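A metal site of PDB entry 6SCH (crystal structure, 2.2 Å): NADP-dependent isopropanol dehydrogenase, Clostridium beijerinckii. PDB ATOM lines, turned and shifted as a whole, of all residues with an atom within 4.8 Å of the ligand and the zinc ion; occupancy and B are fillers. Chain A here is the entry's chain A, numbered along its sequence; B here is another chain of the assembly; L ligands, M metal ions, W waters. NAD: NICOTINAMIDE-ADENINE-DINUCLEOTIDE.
O of Lys 340 lies within hydrogen-bond range of NH1 of Arg 200, 3.4 Å away. ND2 of Asn 266 lies within hydrogen-bond range of O of Gly 244 (2.7 Å). The backbone carbonyl oxygen (O) of Met 285 of chain B sits at hydrogen-bond distance from the backbone NH (N) of Leu 294, 3.1 Å away. N of Gly 174 is in hydrogen-bond range of O of Val 197 (2.8 Å). N of Arg 200 lies within hydrogen-bond range of OD2 of Asp 198, at 3.1 Å. N of Gly 243 is in hydrogen-bond range of O of Ile 173 (2.9 Å). N of Ala 242 is in hydrogen-bond range of O of Ile 173, at 2.9 Å. The side-chain carboxylate of Asp 198 lies within hydrogen-bond range of the backbone NH of Ile 175 (2.7 Å).
OG of Ser 39 touches the zinc ion (3.4 Å). Four residues have an atom within 4 Å of the zinc ion: Cys 37, Ser 39, His 59 and Asp 150.
The backbone carbonyl oxygen (O) of Ile 265 sits close to an oxygen (O4D) of the ligand (3.4 Å). OG of Ser 39 touches N7N of the ligand, at 3.6 Å. Met 151 touches the ligand. OG1 of Thr 154 touches C4N of the ligand, 3.7 Å away. CG2 of Ile 173 touches C2A of the ligand (3.8 Å). CA of Gly 174 touches O4B of the ligand, at 3.4 Å. Gly 176 touches the ligand. Val 197 touches the ligand (O to N3A, 3.8 Å). Arg 200 touches the ligand. Ala 242 touches the ligand (O to C5D, 3.1 Å). Gly 243 touches the ligand. CA of Gly 244 touches N7A of the ligand, 3.2 Å away. Tyr 267 touches the ligand. CD1 of Leu 294 touches O7N of the ligand (3.3 Å). CD of Lys 340 touches O1A of the ligand (3.6 Å). Hydrophobic or aromatic side chains within 4 Å of the ligand: His 42, His 59, Met 151, Ile 173, Val 178, Tyr 199, Tyr 267 and Leu 294.
The zinc ion is bound by OD2 of Asp 150 (2.0 Å), NE2 of His 59 (2.0 Å), SG of Cys 37 (2.4 Å) and N7N of the ligand (2.6 Å).
Water W1 lies within hydrogen-bond range of O1N of the ligand (2.9 Å) and N of Thr 38 (3.2 Å). Water W2 lies within hydrogen-bond range of O7N of the ligand (3.0 Å) and OG1 of Thr 154 (3.1 Å).
The backbone NH of Ala 177 lies within hydrogen-bond range of an oxygen (O2N) of the ligand (3.5 Å). The side-chain carboxylate (OD2) of Asp 198 sits at hydrogen-bond distance from an oxygen (O2B) of the ligand (3.2 Å). A nitrogen (N6A) of the ligand sits at hydrogen-bond distance from the side-chain carboxylate (OE2) of Glu 247. NE2 of His 42 is in hydrogen-bond range of O3D of the ligand (3.4 Å). OD1 of Asn 266 sits at hydrogen-bond distance from O3D of the ligand. An oxygen (O2B) of the ligand lies close to the side-chain hydroxyl (OH) of Tyr 199 (3.1 Å). The backbone NH (N) of Val 178 is in hydrogen-bond range of an oxygen (O2N) of the ligand (3.4 Å). O5D of the ligand lies close to OG1 of Thr 38 (3.4 Å).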
ATOM      1  N   CYS A  37      14.065 -25.982   6.969  1.00  0.00           N
ATOM      2  CA  CYS A  37      15.339 -25.331   6.671  1.00  0.00           C
ATOM      3  C   CYS A  37      15.673 -24.366   7.799  1.00  0.00           C
ATOM      4  O   CYS A  37      14.776 -23.816   8.440  1.00  0.00           O
ATOM      5  CB  CYS A  37      15.263 -24.587   5.335  1.00  0.00           C
ATOM      6  SG  CYS A  37      16.806 -23.817   4.779  1.00  0.00           S
ATOM      7  N   THR A  38      16.972 -24.191   8.087  1.00  0.00           N
ATOM      8  CA  THR A  38      17.356 -23.196   9.089  1.00  0.00           C
ATOM      9  C   THR A  38      16.963 -21.774   8.681  1.00  0.00           C
ATOM     10  O   THR A  38      16.823 -20.910   9.542  1.00  0.00           O
ATOM     11  CB  THR A  38      18.860 -23.253   9.361  1.00  0.00           C
ATOM     12  OG1 THR A  38      19.582 -22.945   8.162  1.00  0.00           O
ATOM     13  CG2 THR A  38      19.259 -24.618   9.855  1.00  0.00           C
ATOM     14  N   SER A  39      16.777 -21.514   7.389  1.00  0.00           N
ATOM     15  CA  SER A  39      16.391 -20.177   6.973  1.00  0.00           C
ATOM     16  C   SER A  39      15.053 -19.775   7.572  1.00  0.00           C
ATOM     17  O   SER A  39      14.845 -18.603   7.900  1.00  0.00           O
ATOM     18  CB  SER A  39      16.357 -20.089   5.456  1.00  0.00           C
ATOM     19  OG  SER A  39      15.358 -20.934   4.938  1.00  0.00           O
ATOM     20  N   HIS A  42      15.806 -18.316  11.067  1.00  0.00           N
ATOM     21  CA  HIS A  42      16.217 -16.913  10.970  1.00  0.00           C
ATOM     22  C   HIS A  42      15.009 -16.036  10.723  1.00  0.00           C
ATOM     23  O   HIS A  42      14.826 -15.000  11.382  1.00  0.00           O
ATOM     24  CB  HIS A  42      17.222 -16.724   9.826  1.00  0.00           C
ATOM     25  CG  HIS A  42      18.544 -17.401  10.042  1.00  0.00           C
ATOM     26  ND1 HIS A  42      19.342 -17.162  11.140  1.00  0.00           N
ATOM     27  CD2 HIS A  42      19.222 -18.282   9.269  1.00  0.00           C
ATOM     28  CE1 HIS A  42      20.449 -17.887  11.040  1.00  0.00           C
ATOM     29  NE2 HIS A  42      20.401 -18.568   9.914  1.00  0.00           N
ATOM     30  N   HIS A  59       9.931 -24.576   2.400  1.00  0.00           N
ATOM     31  CA  HIS A  59      10.161 -24.445   0.957  1.00  0.00           C
ATOM     32  C   HIS A  59      10.909 -25.643   0.361  1.00  0.00           C
ATOM     33  O   HIS A  59      11.450 -25.520  -0.741  1.00  0.00           O
ATOM     34  CB  HIS A  59      10.924 -23.151   0.647  1.00  0.00           C
ATOM     35  CG  HIS A  59      12.178 -22.970   1.438  1.00  0.00           C
ATOM     36  ND1 HIS A  59      12.242 -22.146   2.532  1.00  0.00           N
ATOM     37  CD2 HIS A  59      13.410 -23.512   1.298  1.00  0.00           C
ATOM     38  CE1 HIS A  59      13.467 -22.179   3.035  1.00  0.00           C
ATOM     39  NE2 HIS A  59      14.188 -23.008   2.306  1.00  0.00           N
ATOM     40  N   GLU A  60      10.937 -26.786   1.036  1.00  0.00           N
ATOM     41  CA  GLU A  60      11.575 -27.993   0.512  1.00  0.00           C
ATOM     42  C   GLU A  60      10.518 -29.091   0.449  1.00  0.00           C
ATOM     43  O   GLU A  60      10.124 -29.641   1.486  1.00  0.00           O
ATOM     44  CB  GLU A  60      12.745 -28.431   1.386  1.00  0.00           C
ATOM     45  CG  GLU A  60      13.847 -27.371   1.501  1.00  0.00           C
ATOM     46  CD  GLU A  60      14.936 -27.721   2.544  1.00  0.00           C
ATOM     47  OE1 GLU A  60      15.774 -28.627   2.318  1.00  0.00           O
ATOM     48  OE2 GLU A  60      14.927 -27.077   3.612  1.00  0.00           O
ATOM     49  N   TRP A 110      12.976 -16.588  -4.867  1.00  0.00           N
ATOM     50  CA  TRP A 110      12.687 -17.464  -3.746  1.00  0.00           C
ATOM     51  C   TRP A 110      11.413 -16.948  -3.092  1.00  0.00           C
ATOM     52  O   TRP A 110      11.442 -15.975  -2.333  1.00  0.00           O
ATOM     53  CB  TRP A 110      13.858 -17.473  -2.769  1.00  0.00           C
ATOM     54  CG  TRP A 110      13.511 -18.047  -1.453  1.00  0.00           C
ATOM     55  CD1 TRP A 110      12.737 -19.140  -1.203  1.00  0.00           C
ATOM     56  CD2 TRP A 110      13.887 -17.518  -0.168  1.00  0.00           C
ATOM     57  NE1 TRP A 110      12.630 -19.352   0.154  1.00  0.00           N
ATOM     58  CE2 TRP A 110      13.328 -18.365   0.809  1.00  0.00           C
ATOM     59  CE3 TRP A 110      14.654 -16.413   0.235  1.00  0.00           C
ATOM     60  CZ2 TRP A 110      13.503 -18.146   2.164  1.00  0.00           C
ATOM     61  CZ3 TRP A 110      14.831 -16.208   1.587  1.00  0.00           C
ATOM     62  CH2 TRP A 110      14.257 -17.067   2.538  1.00  0.00           C
ATOM     63  N   ASP A 150      16.783 -27.838  -2.335  1.00  0.00           N
ATOM     64  CA  ASP A 150      17.430 -26.724  -1.635  1.00  0.00           C
ATOM     65  C   ASP A 150      18.867 -27.078  -1.245  1.00  0.00           C
ATOM     66  O   ASP A 150      19.816 -26.418  -1.683  1.00  0.00           O
ATOM     67  CB  ASP A 150      16.577 -26.346  -0.426  1.00  0.00           C
ATOM     68  CG  ASP A 150      17.091 -25.133   0.330  1.00  0.00           C
ATOM     69  OD1 ASP A 150      18.126 -24.561  -0.052  1.00  0.00           O
ATOM     70  OD2 ASP A 150      16.443 -24.763   1.329  1.00  0.00           O
ATOM     71  N   MET A 151      19.047 -28.125  -0.444  1.00  0.00           N
ATOM     72  CA  MET A 151      20.385 -28.480   0.024  1.00  0.00           C
ATOM     73  C   MET A 151      21.332 -28.696  -1.152  1.00  0.00           C
ATOM     74  O   MET A 151      22.383 -28.058  -1.227  1.00  0.00           O
ATOM     75  CB  MET A 151      20.302 -29.713   0.910  1.00  0.00           C
ATOM     76  CG  MET A 151      19.502 -29.508   2.187  1.00  0.00           C
ATOM     77  SD  MET A 151      20.116 -28.138   3.225  1.00  0.00           S
ATOM     78  CE  MET A 151      18.960 -26.824   2.812  1.00  0.00           C
ATOM     79  N   THR A 154      21.776 -25.421  -3.405  1.00  0.00           N
ATOM     80  CA  THR A 154      22.506 -24.364  -2.696  1.00  0.00           C
ATOM     81  C   THR A 154      23.971 -24.728  -2.518  1.00  0.00           C
ATOM     82  O   THR A 154      24.866 -23.949  -2.872  1.00  0.00           O
ATOM     83  CB  THR A 154      21.858 -24.116  -1.321  1.00  0.00           C
ATOM     84  OG1 THR A 154      20.513 -23.676  -1.489  1.00  0.00           O
ATOM     85  CG2 THR A 154      22.654 -23.075  -0.499  1.00  0.00           C
ATOM     86  N   ILE A 173      33.610 -23.749   5.337  1.00  0.00           N
ATOM     87  CA  ILE A 173      33.360 -23.347   6.712  1.00  0.00           C
ATOM     88  C   ILE A 173      31.892 -23.632   7.034  1.00  0.00           C
ATOM     89  O   ILE A 173      30.991 -23.080   6.397  1.00  0.00           O
ATOM     90  CB  ILE A 173      33.714 -21.871   6.953  1.00  0.00           C
ATOM     91  CG1 ILE A 173      35.175 -21.612   6.572  1.00  0.00           C
ATOM     92  CG2 ILE A 173      33.464 -21.487   8.417  1.00  0.00           C
ATOM     93  CD1 ILE A 173      35.546 -20.123   6.586  1.00  0.00           C
ATOM     94  N   GLY A 174      31.654 -24.483   8.016  1.00  0.00           N
ATOM     95  CA  GLY A 174      30.305 -24.908   8.316  1.00  0.00           C
ATOM     96  C   GLY A 174      29.935 -26.154   7.549  1.00  0.00           C
ATOM     97  O   GLY A 174      29.742 -26.095   6.331  1.00  0.00           O
ATOM     98  N   ILE A 175      29.815 -27.269   8.252  1.00  0.00           N
ATOM     99  CA  ILE A 175      29.578 -28.565   7.620  1.00  0.00           C
ATOM    100  C   ILE A 175      28.217 -29.110   8.028  1.00  0.00           C
ATOM    101  O   ILE A 175      28.060 -30.313   8.250  1.00  0.00           O
ATOM    102  CB  ILE A 175      30.700 -29.551   7.981  1.00  0.00           C
ATOM    103  CG1 ILE A 175      32.048 -28.872   7.842  1.00  0.00           C
ATOM    104  CG2 ILE A 175      30.715 -30.710   7.019  1.00  0.00           C
ATOM    105  CD1 ILE A 175      32.279 -28.342   6.437  1.00  0.00           C
ATOM    106  N   GLY A 176      27.220 -28.242   8.124  1.00  0.00           N
ATOM    107  CA  GLY A 176      25.849 -28.678   8.099  1.00  0.00           C
ATOM    108  C   GLY A 176      25.469 -29.171   6.705  1.00  0.00           C
ATOM    109  O   GLY A 176      26.287 -29.315   5.797  1.00  0.00           O
ATOM    110  N   ALA A 177      24.159 -29.364   6.527  1.00  0.00           N
ATOM    111  CA  ALA A 177      23.647 -29.892   5.272  1.00  0.00           C
ATOM    112  C   ALA A 177      24.158 -29.114   4.076  1.00  0.00           C
ATOM    113  O   ALA A 177      24.687 -29.689   3.125  1.00  0.00           O
ATOM    114  CB  ALA A 177      22.117 -29.874   5.311  1.00  0.00           C
ATOM    115  N   VAL A 178      24.048 -27.776   4.130  1.00  0.00           N
ATOM    116  CA  VAL A 178      24.472 -26.945   3.016  1.00  0.00           C
ATOM    117  C   VAL A 178      25.963 -27.100   2.775  1.00  0.00           C
ATOM    118  O   VAL A 178      26.412 -27.255   1.634  1.00  0.00           O
ATOM    119  CB  VAL A 178      24.054 -25.483   3.250  1.00  0.00           C
ATOM    120  CG1 VAL A 178      24.693 -24.545   2.239  1.00  0.00           C
ATOM    121  CG2 VAL A 178      22.546 -25.363   3.174  1.00  0.00           C
ATOM    122  N   GLY A 179      26.768 -27.076   3.848  1.00  0.00           N
ATOM    123  CA  GLY A 179      28.203 -27.286   3.713  1.00  0.00           C
ATOM    124  C   GLY A 179      28.598 -28.671   3.220  1.00  0.00           C
ATOM    125  O   GLY A 179      29.587 -28.822   2.495  1.00  0.00           O
ATOM    126  N   VAL A 197      35.456 -27.279   8.157  1.00  0.00           N
ATOM    127  CA  VAL A 197      35.605 -26.611   9.457  1.00  0.00           C
ATOM    128  C   VAL A 197      34.268 -26.652  10.167  1.00  0.00           C
ATOM    129  O   VAL A 197      33.294 -26.043   9.717  1.00  0.00           O
ATOM    130  CB  VAL A 197      36.117 -25.181   9.334  1.00  0.00           C
ATOM    131  CG1 VAL A 197      36.347 -24.598  10.734  1.00  0.00           C
ATOM    132  CG2 VAL A 197      37.384 -25.129   8.527  1.00  0.00           C
ATOM    133  N   ASP A 198      34.233 -27.337  11.313  1.00  0.00           N
ATOM    134  CA  ASP A 198      33.016 -27.485  12.104  1.00  0.00           C
ATOM    135  C   ASP A 198      33.395 -28.179  13.409  1.00  0.00           C
ATOM    136  O   ASP A 198      34.507 -28.663  13.579  1.00  0.00           O
ATOM    137  CB  ASP A 198      31.951 -28.291  11.360  1.00  0.00           C
ATOM    138  CG  ASP A 198      30.542 -27.863  11.723  1.00  0.00           C
ATOM    139  OD1 ASP A 198      29.907 -27.138  10.923  1.00  0.00           O
ATOM    140  OD2 ASP A 198      30.055 -28.252  12.813  1.00  0.00           O
ATOM    141  N   TYR A 199      32.411 -28.247  14.313  1.00  0.00           N
ATOM    142  CA  TYR A 199      32.578 -28.869  15.620  1.00  0.00           C
ATOM    143  C   TYR A 199      31.587 -29.989  15.911  1.00  0.00           C
ATOM    144  O   TYR A 199      31.606 -30.524  17.033  1.00  0.00           O
ATOM    145  CB  TYR A 199      32.487 -27.802  16.729  1.00  0.00           C
ATOM    146  CG  TYR A 199      31.249 -26.937  16.618  1.00  0.00           C
ATOM    147  CD1 TYR A 199      30.026 -27.349  17.138  1.00  0.00           C
ATOM    148  CD2 TYR A 199      31.326 -25.677  16.029  1.00  0.00           C
ATOM    149  CE1 TYR A 199      28.902 -26.542  17.039  1.00  0.00           C
ATOM    150  CE2 TYR A 199      30.219 -24.866  15.929  1.00  0.00           C
ATOM    151  CZ  TYR A 199      29.008 -25.301  16.427  1.00  0.00           C
ATOM    152  OH  TYR A 199      27.904 -24.482  16.325  1.00  0.00           O
ATOM    153  N   ARG A 200      30.743 -30.378  14.958  1.00  0.00           N
ATOM    154  CA  ARG A 200      29.703 -31.366  15.240  1.00  0.00           C
ATOM    155  C   ARG A 200      30.113 -32.738  14.736  1.00  0.00           C
ATOM    156  O   ARG A 200      30.355 -32.902  13.528  1.00  0.00           O
ATOM    157  CB  ARG A 200      28.376 -30.939  14.615  1.00  0.00           C
ATOM    158  CG  ARG A 200      27.824 -29.664  15.226  1.00  0.00           C
ATOM    159  CD  ARG A 200      26.601 -29.135  14.497  1.00  0.00           C
ATOM    160  NE  ARG A 200      25.467 -30.060  14.589  1.00  0.00           N
ATOM    161  CZ  ARG A 200      24.603 -30.071  15.591  1.00  0.00           C
ATOM    162  NH1 ARG A 200      24.708 -29.204  16.591  1.00  0.00           N
ATOM    163  NH2 ARG A 200      23.604 -30.948  15.592  1.00  0.00           N
ATOM    164  N   CYS A 203      28.526 -34.615  11.561  1.00  0.00           N
ATOM    165  CA  CYS A 203      28.900 -34.083  10.260  1.00  0.00           C
ATOM    166  C   CYS A 203      30.252 -34.585   9.800  1.00  0.00           C
ATOM    167  O   CYS A 203      30.524 -34.567   8.599  1.00  0.00           O
ATOM    168  CB  CYS A 203      28.907 -32.552  10.331  1.00  0.00           C
ATOM    169  SG  CYS A 203      27.300 -31.857  10.832  1.00  0.00           S
ATOM    170  N   PRO A 218      37.246 -25.639  15.350  1.00  0.00           N
ATOM    171  CA  PRO A 218      37.698 -24.356  15.916  1.00  0.00           C
ATOM    172  C   PRO A 218      37.948 -24.408  17.418  1.00  0.00           C
ATOM    173  O   PRO A 218      38.683 -23.571  17.939  1.00  0.00           O
ATOM    174  CB  PRO A 218      36.546 -23.395  15.577  1.00  0.00           C
ATOM    175  CG  PRO A 218      35.790 -24.061  14.445  1.00  0.00           C
ATOM    176  CD  PRO A 218      35.937 -25.540  14.687  1.00  0.00           C
ATOM    177  N   ALA A 242      29.568 -21.622   4.346  1.00  0.00           N
ATOM    178  CA  ALA A 242      28.292 -22.318   4.391  1.00  0.00           C
ATOM    179  C   ALA A 242      27.642 -22.298   5.760  1.00  0.00           C
ATOM    180  O   ALA A 242      26.450 -22.595   5.855  1.00  0.00           O
ATOM    181  CB  ALA A 242      28.468 -23.779   3.926  1.00  0.00           C
ATOM    182  N   GLY A 243      28.368 -21.953   6.804  1.00  0.00           N
ATOM    183  CA  GLY A 243      27.720 -21.844   8.099  1.00  0.00           C
ATOM    184  C   GLY A 243      28.574 -21.074   9.082  1.00  0.00           C
ATOM    185  O   GLY A 243      29.764 -20.858   8.872  1.00  0.00           O
ATOM    186  N   GLY A 244      27.934 -20.678  10.177  1.00  0.00           N
ATOM    187  CA  GLY A 244      28.574 -19.873  11.188  1.00  0.00           C
ATOM    188  C   GLY A 244      28.179 -18.416  11.075  1.00  0.00           C
ATOM    189  O   GLY A 244      27.452 -18.000  10.172  1.00  0.00           O
ATOM    190  N   GLY A 245      28.719 -17.620  11.987  1.00  0.00           N
ATOM    191  CA  GLY A 245      28.365 -16.223  12.068  1.00  0.00           C
ATOM    192  C   GLY A 245      29.117 -15.393  11.054  1.00  0.00           C
ATOM    193  O   GLY A 245      29.891 -15.888  10.231  1.00  0.00           O
ATOM    194  N   GLU A 247      31.575 -13.448  11.371  1.00  0.00           N
ATOM    195  CA  GLU A 247      33.023 -13.399  11.501  1.00  0.00           C
ATOM    196  C   GLU A 247      33.740 -14.412  10.617  1.00  0.00           C
ATOM    197  O   GLU A 247      34.960 -14.300  10.444  1.00  0.00           O
ATOM    198  CB  GLU A 247      33.415 -13.561  12.965  1.00  0.00           C
ATOM    199  CG  GLU A 247      33.338 -14.990  13.447  1.00  0.00           C
ATOM    200  CD  GLU A 247      31.904 -15.398  13.790  1.00  0.00           C
ATOM    201  OE1 GLU A 247      30.989 -14.546  13.694  1.00  0.00           O
ATOM    202  OE2 GLU A 247      31.709 -16.581  14.131  1.00  0.00           O
ATOM    203  N   THR A 248      33.031 -15.394  10.034  1.00  0.00           N
ATOM    204  CA  THR A 248      33.699 -16.319   9.140  1.00  0.00           C
ATOM    205  C   THR A 248      34.191 -15.648   7.867  1.00  0.00           C
ATOM    206  O   THR A 248      35.095 -16.181   7.220  1.00  0.00           O
ATOM    207  CB  THR A 248      32.768 -17.480   8.762  1.00  0.00           C
ATOM    208  OG1 THR A 248      31.598 -16.971   8.117  1.00  0.00           O
ATOM    209  CG2 THR A 248      32.393 -18.304  10.003  1.00  0.00           C
ATOM    210  N   ILE A 265      27.300 -18.933   0.597  1.00  0.00           N
ATOM    211  CA  ILE A 265      25.942 -19.410   0.460  1.00  0.00           C
ATOM    212  C   ILE A 265      25.199 -19.378   1.775  1.00  0.00           C
ATOM    213  O   ILE A 265      24.018 -19.728   1.821  1.00  0.00           O
ATOM    214  CB  ILE A 265      25.917 -20.832  -0.126  1.00  0.00           C
ATOM    215  CG1 ILE A 265      26.902 -21.719   0.650  1.00  0.00           C
ATOM    216  CG2 ILE A 265      26.246 -20.771  -1.584  1.00  0.00           C
ATOM    217  CD1 ILE A 265      27.088 -23.113   0.015  1.00  0.00           C
ATOM    218  N   ASN A 266      25.877 -18.950   2.833  1.00  0.00           N
ATOM    219  CA  ASN A 266      25.305 -18.808   4.159  1.00  0.00           C
ATOM    220  C   ASN A 266      24.368 -17.611   4.192  1.00  0.00           C
ATOM    221  O   ASN A 266      24.667 -16.539   3.641  1.00  0.00           O
ATOM    222  CB  ASN A 266      26.432 -18.672   5.175  1.00  0.00           C
ATOM    223  CG  ASN A 266      25.974 -18.817   6.617  1.00  0.00           C
ATOM    224  OD1 ASN A 266      24.830 -19.178   6.900  1.00  0.00           O
ATOM    225  ND2 ASN A 266      26.895 -18.560   7.544  1.00  0.00           N
ATOM    226  N   TYR A 267      23.203 -17.797   4.789  1.00  0.00           N
ATOM    227  CA  TYR A 267      22.222 -16.732   4.955  1.00  0.00           C
ATOM    228  C   TYR A 267      22.564 -16.023   6.259  1.00  0.00           C
ATOM    229  O   TYR A 267      22.428 -16.606   7.335  1.00  0.00           O
ATOM    230  CB  TYR A 267      20.829 -17.356   4.916  1.00  0.00           C
ATOM    231  CG  TYR A 267      19.578 -16.617   5.370  1.00  0.00           C
ATOM    232  CD1 TYR A 267      19.610 -15.402   6.070  1.00  0.00           C
ATOM    233  CD2 TYR A 267      18.330 -17.174   5.094  1.00  0.00           C
ATOM    234  CE1 TYR A 267      18.441 -14.773   6.468  1.00  0.00           C
ATOM    235  CE2 TYR A 267      17.160 -16.568   5.492  1.00  0.00           C
ATOM    236  CZ  TYR A 267      17.213 -15.367   6.175  1.00  0.00           C
ATOM    237  OH  TYR A 267      16.029 -14.773   6.547  1.00  0.00           O
ATOM    238  N   LEU A 294      21.924 -16.605  -3.647  1.00  0.00           N
ATOM    239  CA  LEU A 294      20.774 -17.485  -3.541  1.00  0.00           C
ATOM    240  C   LEU A 294      20.840 -18.591  -4.593  1.00  0.00           C
ATOM    241  O   LEU A 294      21.270 -18.370  -5.719  1.00  0.00           O
ATOM    242  CB  LEU A 294      19.517 -16.645  -3.726  1.00  0.00           C
ATOM    243  CG  LEU A 294      18.172 -17.334  -3.792  1.00  0.00           C
ATOM    244  CD1 LEU A 294      17.909 -18.068  -2.470  1.00  0.00           C
ATOM    245  CD2 LEU A 294      17.106 -16.269  -4.042  1.00  0.00           C
ATOM    246  N   MET A 337      15.400 -27.891  14.058  1.00  0.00           N
ATOM    247  CA  MET A 337      16.372 -27.007  13.419  1.00  0.00           C
ATOM    248  C   MET A 337      16.743 -25.806  14.298  1.00  0.00           C
ATOM    249  O   MET A 337      17.787 -25.182  14.063  1.00  0.00           O
ATOM    250  CB  MET A 337      15.831 -26.513  12.081  1.00  0.00           C
ATOM    251  CG  MET A 337      15.513 -27.640  11.113  1.00  0.00           C
ATOM    252  SD  MET A 337      16.885 -28.797  10.842  1.00  0.00           S
ATOM    253  CE  MET A 337      17.751 -27.899   9.551  1.00  0.00           C
ATOM    254  N   LYS A 340      18.847 -28.018  17.303  1.00  0.00           N
ATOM    255  CA  LYS A 340      19.942 -28.764  16.679  1.00  0.00           C
ATOM    256  C   LYS A 340      20.613 -29.742  17.633  1.00  0.00           C
ATOM    257  O   LYS A 340      21.696 -29.455  18.155  1.00  0.00           O
ATOM    258  CB  LYS A 340      20.961 -27.766  16.146  1.00  0.00           C
ATOM    259  CG  LYS A 340      20.603 -27.164  14.797  1.00  0.00           C
ATOM    260  CD  LYS A 340      21.465 -25.945  14.495  1.00  0.00           C
ATOM    261  CE  LYS A 340      21.255 -24.882  15.569  1.00  0.00           C
ATOM    262  NZ  LYS A 340      22.049 -23.642  15.309  1.00  0.00           N
ATOM    263  N   MET B 285      23.144 -13.119  -0.208  1.00  0.00           N
ATOM    264  CA  MET B 285      22.576 -13.909  -1.288  1.00  0.00           C
ATOM    265  C   MET B 285      22.175 -13.076  -2.507  1.00  0.00           C
ATOM    266  O   MET B 285      21.463 -13.574  -3.365  1.00  0.00           O
ATOM    267  CB  MET B 285      21.381 -14.703  -0.751  1.00  0.00           C
ATOM    268  CG  MET B 285      21.770 -15.790   0.254  1.00  0.00           C
ATOM    269  SD  MET B 285      20.363 -16.620   1.031  1.00  0.00           S
ATOM    270  CE  MET B 285      19.005 -15.543   0.589  1.00  0.00           C
HETATM  271  PA  NAD L   1      23.310 -25.047  10.210  1.00  0.00           P
HETATM  272  O1A NAD L   1      22.392 -24.523  11.284  1.00  0.00           O
HETATM  273  O2A NAD L   1      23.509 -26.532  10.031  1.00  0.00           O
HETATM  274  O5B NAD L   1      24.749 -24.367  10.456  1.00  0.00           O
HETATM  275  C5B NAD L   1      25.840 -24.795   9.643  1.00  0.00           C
HETATM  276  C4B NAD L   1      26.948 -25.437  10.470  1.00  0.00           C
HETATM  277  O4B NAD L   1      27.952 -24.476  10.785  1.00  0.00           O
HETATM  278  C3B NAD L   1      26.460 -26.041  11.781  1.00  0.00           C
HETATM  279  O3B NAD L   1      26.695 -27.461  11.754  1.00  0.00           O
HETATM  280  C2B NAD L   1      27.268 -25.346  12.861  1.00  0.00           C
HETATM  281  O2B NAD L   1      27.732 -26.266  13.851  1.00  0.00           O
HETATM  282  C1B NAD L   1      28.434 -24.730  12.113  1.00  0.00           C
HETATM  283  N9A NAD L   1      28.987 -23.478  12.687  1.00  0.00           N
HETATM  284  C8A NAD L   1      28.354 -22.585  13.488  1.00  0.00           C
HETATM  285  N7A NAD L   1      29.186 -21.567  13.812  1.00  0.00           N
HETATM  286  C5A NAD L   1      30.381 -21.803  13.217  1.00  0.00           C
HETATM  287  C6A NAD L   1      31.701 -21.127  13.136  1.00  0.00           C
HETATM  288  N6A NAD L   1      31.932 -19.960  13.781  1.00  0.00           N
HETATM  289  N1A NAD L   1      32.677 -21.721  12.395  1.00  0.00           N
HETATM  290  C2A NAD L   1      32.462 -22.884  11.750  1.00  0.00           C
HETATM  291  N3A NAD L   1      31.293 -23.552  11.776  1.00  0.00           N
HETATM  292  C4A NAD L   1      30.235 -23.072  12.476  1.00  0.00           C
HETATM  293  O3  NAD L   1      22.867 -24.423   8.775  1.00  0.00           O
HETATM  294  PN  NAD L   1      22.661 -25.240   7.387  1.00  0.00           P
HETATM  295  O1N NAD L   1      21.394 -26.079   7.458  1.00  0.00           O
HETATM  296  O2N NAD L   1      23.940 -25.918   6.952  1.00  0.00           O
HETATM  297  O5D NAD L   1      22.373 -23.969   6.423  1.00  0.00           O
HETATM  298  C5D NAD L   1      23.453 -23.158   5.926  1.00  0.00           C
HETATM  299  C4D NAD L   1      23.072 -21.678   5.828  1.00  0.00           C
HETATM  300  O4D NAD L   1      22.606 -21.335   4.516  1.00  0.00           O
HETATM  301  C3D NAD L   1      21.965 -21.348   6.815  1.00  0.00           C
HETATM  302  O3D NAD L   1      22.358 -20.273   7.686  1.00  0.00           O
HETATM  303  C2D NAD L   1      20.775 -20.976   5.954  1.00  0.00           C
HETATM  304  O2D NAD L   1      20.047 -19.896   6.531  1.00  0.00           O
HETATM  305  C1D NAD L   1      21.336 -20.679   4.563  1.00  0.00           C
HETATM  306  N1N NAD L   1      20.453 -21.246   3.533  1.00  0.00           N
HETATM  307  C2N NAD L   1      19.483 -20.543   2.917  1.00  0.00           C
HETATM  308  C3N NAD L   1      18.690 -21.186   1.954  1.00  0.00           C
HETATM  309  C7N NAD L   1      17.567 -20.552   1.189  1.00  0.00           C
HETATM  310  O7N NAD L   1      17.786 -19.710   0.336  1.00  0.00           O
HETATM  311  N7N NAD L   1      16.338 -20.959   1.460  1.00  0.00           N
HETATM  312  C4N NAD L   1      18.907 -22.523   1.690  1.00  0.00           C
HETATM  313  C5N NAD L   1      19.904 -23.214   2.348  1.00  0.00           C
HETATM  314  C6N NAD L   1      20.665 -22.535   3.274  1.00  0.00           C
HETATM  315 ZN    ZN M   1      16.161 -23.286   2.573  1.00  0.00          ZN
HETATM  316 MG    MG M   2      24.832 -21.457  10.576  1.00  0.00          MG
HETATM  317  O   HOH W   1      18.676 -26.281   6.348  1.00  0.00           O
HETATM  318  O   HOH W   2      20.200 -20.598  -1.282  1.00  0.00           O
HETATM  319  O   HOH W   3      24.521 -23.678  13.991  1.00  0.00           O
